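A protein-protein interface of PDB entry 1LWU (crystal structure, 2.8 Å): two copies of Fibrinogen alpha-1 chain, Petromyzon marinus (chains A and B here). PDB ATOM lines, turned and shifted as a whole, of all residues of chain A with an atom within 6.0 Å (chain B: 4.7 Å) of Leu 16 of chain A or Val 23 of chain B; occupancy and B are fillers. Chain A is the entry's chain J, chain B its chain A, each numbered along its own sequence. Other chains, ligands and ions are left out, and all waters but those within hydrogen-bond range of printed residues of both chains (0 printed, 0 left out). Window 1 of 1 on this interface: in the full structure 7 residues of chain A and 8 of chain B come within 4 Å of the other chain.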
ATOM      1  N   ASN A  14      -6.528 -21.708  15.619  1.00  0.00           N
ATOM      2  CA  ASN A  14      -6.834 -21.852  14.168  1.00  0.00           C
ATOM      3  C   ASN A  14      -7.812 -20.775  13.693  1.00  0.00           C
ATOM      4  O   ASN A  14      -8.372 -20.869  12.599  1.00  0.00           O
ATOM      5  CB  ASN A  14      -7.431 -23.231  13.889  1.00  0.00           C
ATOM      6  CG  ASN A  14      -8.830 -23.383  14.450  1.00  0.00           C
ATOM      7  OD1 ASN A  14      -9.039 -23.296  15.659  1.00  0.00           O
ATOM      8  ND2 ASN A  14      -9.801 -23.609  13.569  1.00  0.00           N
ATOM      9  N   GLU A  15      -8.023 -19.760  14.525  1.00  0.00           N
ATOM     10  CA  GLU A  15      -8.918 -18.661  14.182  1.00  0.00           C
ATOM     11  C   GLU A  15      -8.190 -17.711  13.239  1.00  0.00           C
ATOM     12  O   GLU A  15      -8.030 -18.008  12.056  1.00  0.00           O
ATOM     13  CB  GLU A  15      -9.345 -17.913  15.444  1.00  0.00           C
ATOM     14  CG  GLU A  15     -10.313 -18.679  16.331  1.00  0.00           C
ATOM     15  CD  GLU A  15     -11.704 -18.766  15.734  1.00  0.00           C
ATOM     16  OE1 GLU A  15     -12.356 -17.710  15.584  1.00  0.00           O
ATOM     17  OE2 GLU A  15     -12.145 -19.889  15.412  1.00  0.00           O
ATOM     18  N   LEU A  16      -7.744 -16.572  13.760  1.00  0.00           N
ATOM     19  CA  LEU A  16      -7.020 -15.623  12.931  1.00  0.00           C
ATOM     20  C   LEU A  16      -5.840 -16.380  12.351  1.00  0.00           C
ATOM     21  O   LEU A  16      -5.317 -16.017  11.305  1.00  0.00           O
ATOM     22  CB  LEU A  16      -6.504 -14.445  13.757  1.00  0.00           C
ATOM     23  CG  LEU A  16      -7.442 -13.843  14.800  1.00  0.00           C
ATOM     24  CD1 LEU A  16      -6.953 -12.443  15.171  1.00  0.00           C
ATOM     25  CD2 LEU A  16      -8.856 -13.807  14.254  1.00  0.00           C
ATOM     26  N   GLU A  17      -5.429 -17.438  13.046  1.00  0.00           N
ATOM     27  CA  GLU A  17      -4.308 -18.274  12.615  1.00  0.00           C
ATOM     28  C   GLU A  17      -4.268 -18.480  11.096  1.00  0.00           C
ATOM     29  O   GLU A  17      -3.341 -18.027  10.421  1.00  0.00           O
ATOM     30  CB  GLU A  17      -4.364 -19.632  13.334  1.00  0.00           C
ATOM     31  CG  GLU A  17      -3.570 -20.745  12.658  1.00  0.00           C
ATOM     32  CD  GLU A  17      -2.124 -20.367  12.398  1.00  0.00           C
ATOM     33  OE1 GLU A  17      -1.380 -20.144  13.375  1.00  0.00           O
ATOM     34  OE2 GLU A  17      -1.736 -20.292  11.214  1.00  0.00           O
ATOM     35  N   VAL A  18      -5.269 -19.163  10.557  1.00  0.00           N
ATOM     36  CA  VAL A  18      -5.312 -19.393   9.124  1.00  0.00           C
ATOM     37  C   VAL A  18      -5.707 -18.105   8.406  1.00  0.00           C
ATOM     38  O   VAL A  18      -5.208 -17.826   7.316  1.00  0.00           O
ATOM     39  CB  VAL A  18      -6.307 -20.522   8.760  1.00  0.00           C
ATOM     40  CG1 VAL A  18      -6.410 -20.656   7.250  1.00  0.00           C
ATOM     41  CG2 VAL A  18      -5.849 -21.840   9.367  1.00  0.00           C
ATOM     42  N   ARG A  19      -6.593 -17.317   9.018  1.00  0.00           N
ATOM     43  CA  ARG A  19      -7.037 -16.054   8.417  1.00  0.00           C
ATOM     44  C   ARG A  19      -5.805 -15.225   8.068  1.00  0.00           C
ATOM     45  O   ARG A  19      -5.702 -14.657   6.981  1.00  0.00           O
ATOM     46  CB  ARG A  19      -7.925 -15.269   9.394  1.00  0.00           C
ATOM     47  CG  ARG A  19      -8.632 -14.067   8.768  1.00  0.00           C
ATOM     48  CD  ARG A  19      -9.320 -13.209   9.820  1.00  0.00           C
ATOM     49  NE  ARG A  19     -10.116 -14.004  10.752  1.00  0.00           N
ATOM     50  CZ  ARG A  19     -10.777 -13.496  11.790  1.00  0.00           C
ATOM     51  NH1 ARG A  19     -10.738 -12.190  12.027  1.00  0.00           N
ATOM     52  NH2 ARG A  19     -11.463 -14.294  12.600  1.00  0.00           N
ATOM     53  N   TYR A  20      -4.874 -15.171   9.015  1.00  0.00           N
ATOM     54  CA  TYR A  20      -3.618 -14.451   8.865  1.00  0.00           C
ATOM     55  C   TYR A  20      -2.761 -15.218   7.874  1.00  0.00           C
ATOM     56  O   TYR A  20      -2.243 -14.644   6.920  1.00  0.00           O
ATOM     57  CB  TYR A  20      -2.902 -14.376  10.216  1.00  0.00           C
ATOM     58  CG  TYR A  20      -1.430 -14.048  10.133  1.00  0.00           C
ATOM     59  CD1 TYR A  20      -0.990 -12.729   9.995  1.00  0.00           C
ATOM     60  CD2 TYR A  20      -0.469 -15.062  10.200  1.00  0.00           C
ATOM     61  CE1 TYR A  20       0.377 -12.427   9.931  1.00  0.00           C
ATOM     62  CE2 TYR A  20       0.896 -14.773  10.135  1.00  0.00           C
ATOM     63  CZ  TYR A  20       1.311 -13.457  10.002  1.00  0.00           C
ATOM     64  OH  TYR A  20       2.658 -13.172   9.951  1.00  0.00           O
ATOM     65  N   SER A  21      -2.628 -16.521   8.099  1.00  0.00           N
ATOM     66  CA  SER A  21      -1.830 -17.365   7.221  1.00  0.00           C
ATOM     67  C   SER A  21      -2.304 -17.266   5.772  1.00  0.00           C
ATOM     68  O   SER A  21      -1.685 -17.823   4.864  1.00  0.00           O
ATOM     69  CB  SER A  21      -1.881 -18.820   7.688  1.00  0.00           C
ATOM     70  OG  SER A  21      -0.892 -19.597   7.027  1.00  0.00           O
ATOM     71  N   VAL A  23      -3.520 -13.990   4.473  1.00  0.00           N
ATOM     72  CA  VAL A  23      -3.023 -12.674   4.094  1.00  0.00           C
ATOM     73  C   VAL A  23      -1.509 -12.709   3.897  1.00  0.00           C
ATOM     74  O   VAL A  23      -0.872 -11.674   3.706  1.00  0.00           O
ATOM     75  CB  VAL A  23      -3.389 -11.617   5.171  1.00  0.00           C
ATOM     76  CG1 VAL A  23      -3.027 -10.220   4.696  1.00  0.00           C
ATOM     77  CG2 VAL A  23      -4.872 -11.691   5.476  1.00  0.00           C
ATOM     78  N   ARG B  19      -7.609  -7.143   4.988  1.00  0.00           N
ATOM     79  CA  ARG B  19      -7.533  -8.361   5.784  1.00  0.00           C
ATOM     80  C   ARG B  19      -6.525  -8.181   6.917  1.00  0.00           C
ATOM     81  O   ARG B  19      -6.898  -8.159   8.088  1.00  0.00           O
ATOM     82  CB  ARG B  19      -7.102  -9.532   4.908  1.00  0.00           C
ATOM     83  CG  ARG B  19      -7.703  -9.537   3.518  1.00  0.00           C
ATOM     84  CD  ARG B  19      -7.146 -10.699   2.735  1.00  0.00           C
ATOM     85  NE  ARG B  19      -7.445 -10.608   1.314  1.00  0.00           N
ATOM     86  CZ  ARG B  19      -7.097 -11.531   0.426  1.00  0.00           C
ATOM     87  NH1 ARG B  19      -6.438 -12.612   0.822  1.00  0.00           N
ATOM     88  NH2 ARG B  19      -7.407 -11.375  -0.854  1.00  0.00           N
ATOM     89  N   TYR B  20      -5.249  -8.047   6.560  1.00  0.00           N
ATOM     90  CA  TYR B  20      -4.185  -7.869   7.540  1.00  0.00           C
ATOM     91  C   TYR B  20      -4.566  -6.964   8.707  1.00  0.00           C
ATOM     92  O   TYR B  20      -4.782  -7.438   9.822  1.00  0.00           O
ATOM     93  CB  TYR B  20      -2.939  -7.289   6.884  1.00  0.00           C
ATOM     94  CG  TYR B  20      -1.819  -7.024   7.867  1.00  0.00           C
ATOM     95  CD1 TYR B  20      -1.024  -8.072   8.349  1.00  0.00           C
ATOM     96  CD2 TYR B  20      -1.549  -5.729   8.323  1.00  0.00           C
ATOM     97  CE1 TYR B  20       0.015  -7.839   9.255  1.00  0.00           C
ATOM     98  CE2 TYR B  20      -0.512  -5.483   9.232  1.00  0.00           C
ATOM     99  CZ  TYR B  20       0.264  -6.545   9.690  1.00  0.00           C
ATOM    100  OH  TYR B  20       1.293  -6.322  10.576  1.00  0.00           O
ATOM    101  N   SER B  21      -4.640  -5.661   8.449  1.00  0.00           N
ATOM    102  CA  SER B  21      -4.971  -4.697   9.493  1.00  0.00           C
ATOM    103  C   SER B  21      -6.202  -5.033  10.332  1.00  0.00           C
ATOM    104  O   SER B  21      -6.253  -4.685  11.511  1.00  0.00           O
ATOM    105  CB  SER B  21      -5.115  -3.293   8.901  1.00  0.00           C
ATOM    106  OG  SER B  21      -3.842  -2.727   8.643  1.00  0.00           O
ATOM    107  N   GLU B  22      -7.193  -5.700   9.748  1.00  0.00           N
ATOM    108  CA  GLU B  22      -8.374  -6.050  10.527  1.00  0.00           C
ATOM    109  C   GLU B  22      -8.131  -7.339  11.308  1.00  0.00           C
ATOM    110  O   GLU B  22      -8.758  -7.573  12.344  1.00  0.00           O
ATOM    111  CB  GLU B  22      -9.606  -6.199   9.637  1.00  0.00           C
ATOM    112  CG  GLU B  22      -9.641  -7.452   8.805  1.00  0.00           C
ATOM    113  CD  GLU B  22     -11.023  -7.719   8.268  1.00  0.00           C
ATOM    114  OE1 GLU B  22     -11.922  -8.039   9.079  1.00  0.00           O
ATOM    115  OE2 GLU B  22     -11.212  -7.600   7.039  1.00  0.00           O
ATOM    116  N   VAL B  23      -7.229  -8.182  10.806  1.00  0.00           N
ATOM    117  CA  VAL B  23      -6.888  -9.416  11.504  1.00  0.00           C
ATOM    118  C   VAL B  23      -6.047  -8.969  12.690  1.00  0.00           C
ATOM    119  O   VAL B  23      -5.927  -9.681  13.686  1.00  0.00           O
ATOM    120  CB  VAL B  23      -6.051 -10.376  10.625  1.00  0.00           C
ATOM    121  CG1 VAL B  23      -5.460 -11.491  11.479  1.00  0.00           C
ATOM    122  CG2 VAL B  23      -6.926 -10.975   9.533  1.00  0.00           C
ATOM    123  N   LEU B  24      -5.480  -7.768  12.570  1.00  0.00           N
ATOM    124  CA  LEU B  24      -4.654  -7.184  13.619  1.00  0.00           C
ATOM    125  C   LEU B  24      -5.559  -6.587  14.690  1.00  0.00           C
ATOM    126  O   LEU B  24      -5.272  -6.701  15.877  1.00  0.00           O
ATOM    127  CB  LEU B  24      -3.741  -6.101  13.046  1.00  0.00           C
ATOM    128  CG  LEU B  24      -2.347  -6.027  13.674  1.00  0.00           C
ATOM    129  CD1 LEU B  24      -1.589  -7.308  13.356  1.00  0.00           C
ATOM    130  CD2 LEU B  24      -1.588  -4.826  13.140  1.00  0.00           C
ATOM    131  N   ARG B  25      -6.649  -5.948  14.270  1.00  0.00           N
ATOM    132  CA  ARG B  25      -7.602  -5.372  15.217  1.00  0.00           C
ATOM    133  C   ARG B  25      -8.577  -6.477  15.610  1.00  0.00           C
ATOM    134  O   ARG B  25      -9.675  -6.223  16.110  1.00  0.00           O
ATOM    135  CB  ARG B  25      -8.366  -4.202  14.591  1.00  0.00           C
ATOM    136  CG  ARG B  25      -9.265  -4.576  13.423  1.00  0.00           C
ATOM    137  CD  ARG B  25     -10.124  -3.391  12.994  1.00  0.00           C
ATOM    138  NE  ARG B  25      -9.331  -2.194  12.719  1.00  0.00           N
ATOM    139  CZ  ARG B  25      -8.456  -2.080  11.723  1.00  0.00           C
ATOM    140  NH1 ARG B  25      -8.256  -3.095  10.895  1.00  0.00           N
ATOM    141  NH2 ARG B  25      -7.780  -0.950  11.551  1.00  0.00           N
ATOM    142  N   GLU B  26      -8.156  -7.710  15.351  1.00  0.00           N
ATOM    143  CA  GLU B  26      -8.929  -8.897  15.673  1.00  0.00           C
ATOM    144  C   GLU B  26      -8.130  -9.684  16.705  1.00  0.00           C
ATOM    145  O   GLU B  26      -8.606 -10.669  17.270  1.00  0.00           O
ATOM    146  CB  GLU B  26      -9.165  -9.741  14.420  1.00  0.00           C
ATOM    147  CG  GLU B  26      -9.820 -11.083  14.695  1.00  0.00           C
ATOM    148  CD  GLU B  26     -11.133 -10.976  15.447  1.00  0.00           C
ATOM    149  OE1 GLU B  26     -11.647 -12.031  15.880  1.00  0.00           O
ATOM    150  OE2 GLU B  26     -11.648  -9.846  15.599  1.00  0.00           O
ATOM    151  N   LEU B  27      -6.896  -9.247  16.933  1.00  0.00           N
ATOM    152  CA  LEU B  27      -6.048  -9.876  17.929  1.00  0.00           C
ATOM    153  C   LEU B  27      -6.397  -9.194  19.239  1.00  0.00           C
ATOM    154  O   LEU B  27      -6.598  -9.851  20.260  1.00  0.00           O
ATOM    155  CB  LEU B  27      -4.566  -9.652  17.626  1.00  0.00           C
ATOM    156  CG  LEU B  27      -3.758 -10.873  17.188  1.00  0.00           C
ATOM    157  CD1 LEU B  27      -2.279 -10.592  17.402  1.00  0.00           C
ATOM    158  CD2 LEU B  27      -4.174 -12.090  17.996  1.00  0.00           C
ATOM    159  N   ARG B  30      -9.333  -9.975  20.847  1.00  0.00           N
ATOM    160  CA  ARG B  30      -9.160 -11.300  21.422  1.00  0.00           C
ATOM    161  C   ARG B  30      -8.243 -11.253  22.649  1.00  0.00           C
ATOM    162  O   ARG B  30      -8.347 -12.086  23.551  1.00  0.00           O
ATOM    163  CB  ARG B  30      -8.591 -12.263  20.375  1.00  0.00           C
ATOM    164  CG  ARG B  30      -8.437 -13.680  20.901  1.00  0.00           C
ATOM    165  CD  ARG B  30      -8.099 -14.688  19.820  1.00  0.00           C
ATOM    166  NE  ARG B  30      -9.142 -14.776  18.803  1.00  0.00           N
ATOM    167  CZ  ARG B  30      -9.257 -15.780  17.941  1.00  0.00           C
ATOM    168  NH1 ARG B  30      -8.394 -16.787  17.978  1.00  0.00           N
ATOM    169  NH2 ARG B  30     -10.227 -15.770  17.034  1.00  0.00           N
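The guanidinium group (NH2) of Arg 30 of chain B lies within salt-bridge range of the side-chain carboxylate (OE1) of Glu 15 of chain A (3.2 Å). OE1 of Glu 26 of chain B lies within salt-bridge range of NH1 of Arg 19 of chain A, 3.96 Å away.
Val 23 of chain B touches Leu 16 of chain A. CD2 of Leu 16 of chain A touches CG of Glu 26 of chain B, at 2.9 Å. Leu 16 of chain A touches Leu 27 of chain B (CD1 to N, 3.6 Å). Arg 30 of chain B touches Leu 16 of chain A. CD of Arg 19 of chain A touches CG2 of Val 23 of chain B, 3.3 Å away. Val 23 of chain A touches Arg 19 of chain B. Val 23 of chain A touches Tyr 20 of chain B.
Arg 19 of chain A touches Val 23 of chain B, and with the chains exchanged Val 23 of chain A touches Arg 19 of chain B. Val 23 of chain A touches Tyr 20 of chain B, but with the chains exchanged Tyr 20 of chain A does not touch Val 23 of chain B (4.1 Å). Positions printed for both chains: 19, 20, 21 and 23.
Printed residues of chain B that touch a printed residue of chain A: Arg 19, Tyr 20, Val 23, Glu 26, Leu 27 and Arg 30. Along chain B the printed residues that touch a printed residue of chain A span positions 19 to 30. Of the 9 printed residues of chain A, 4 touch a printed residue of chain B. Hydrophobic or aromatic side chains of chain A within 4 Å of the printed part of chain B: Leu 16 and Val 23.
Leu 16 of chain A touches just these residues of chain B: Val 23 (3.3 Å), Glu 26 (2.9 Å), Leu 27 (3.6 Å) and Arg 30 (3.7 Å). Of the printed residues of chain A, Arg 19 of chain B touches Val 23. Of the printed residues of chain A, Glu 26 of chain B touches Leu 16 and Arg 19. Printed residues of chain A within 4 Å of Arg 30 of chain B: Glu 15 and Leu 16. The nearest printed residue of chain B that does not touch Leu 16 of chain A is Leu 24 of chain B (5.5 Å). The nearest residue of chain A that does not touch Val 23 of chain B is Tyr 20 of chain A (4.1 Å). The nearest printed residue of chain A that does not touch Glu 26 of chain B is Glu 15 of chain A (5.7 Å).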
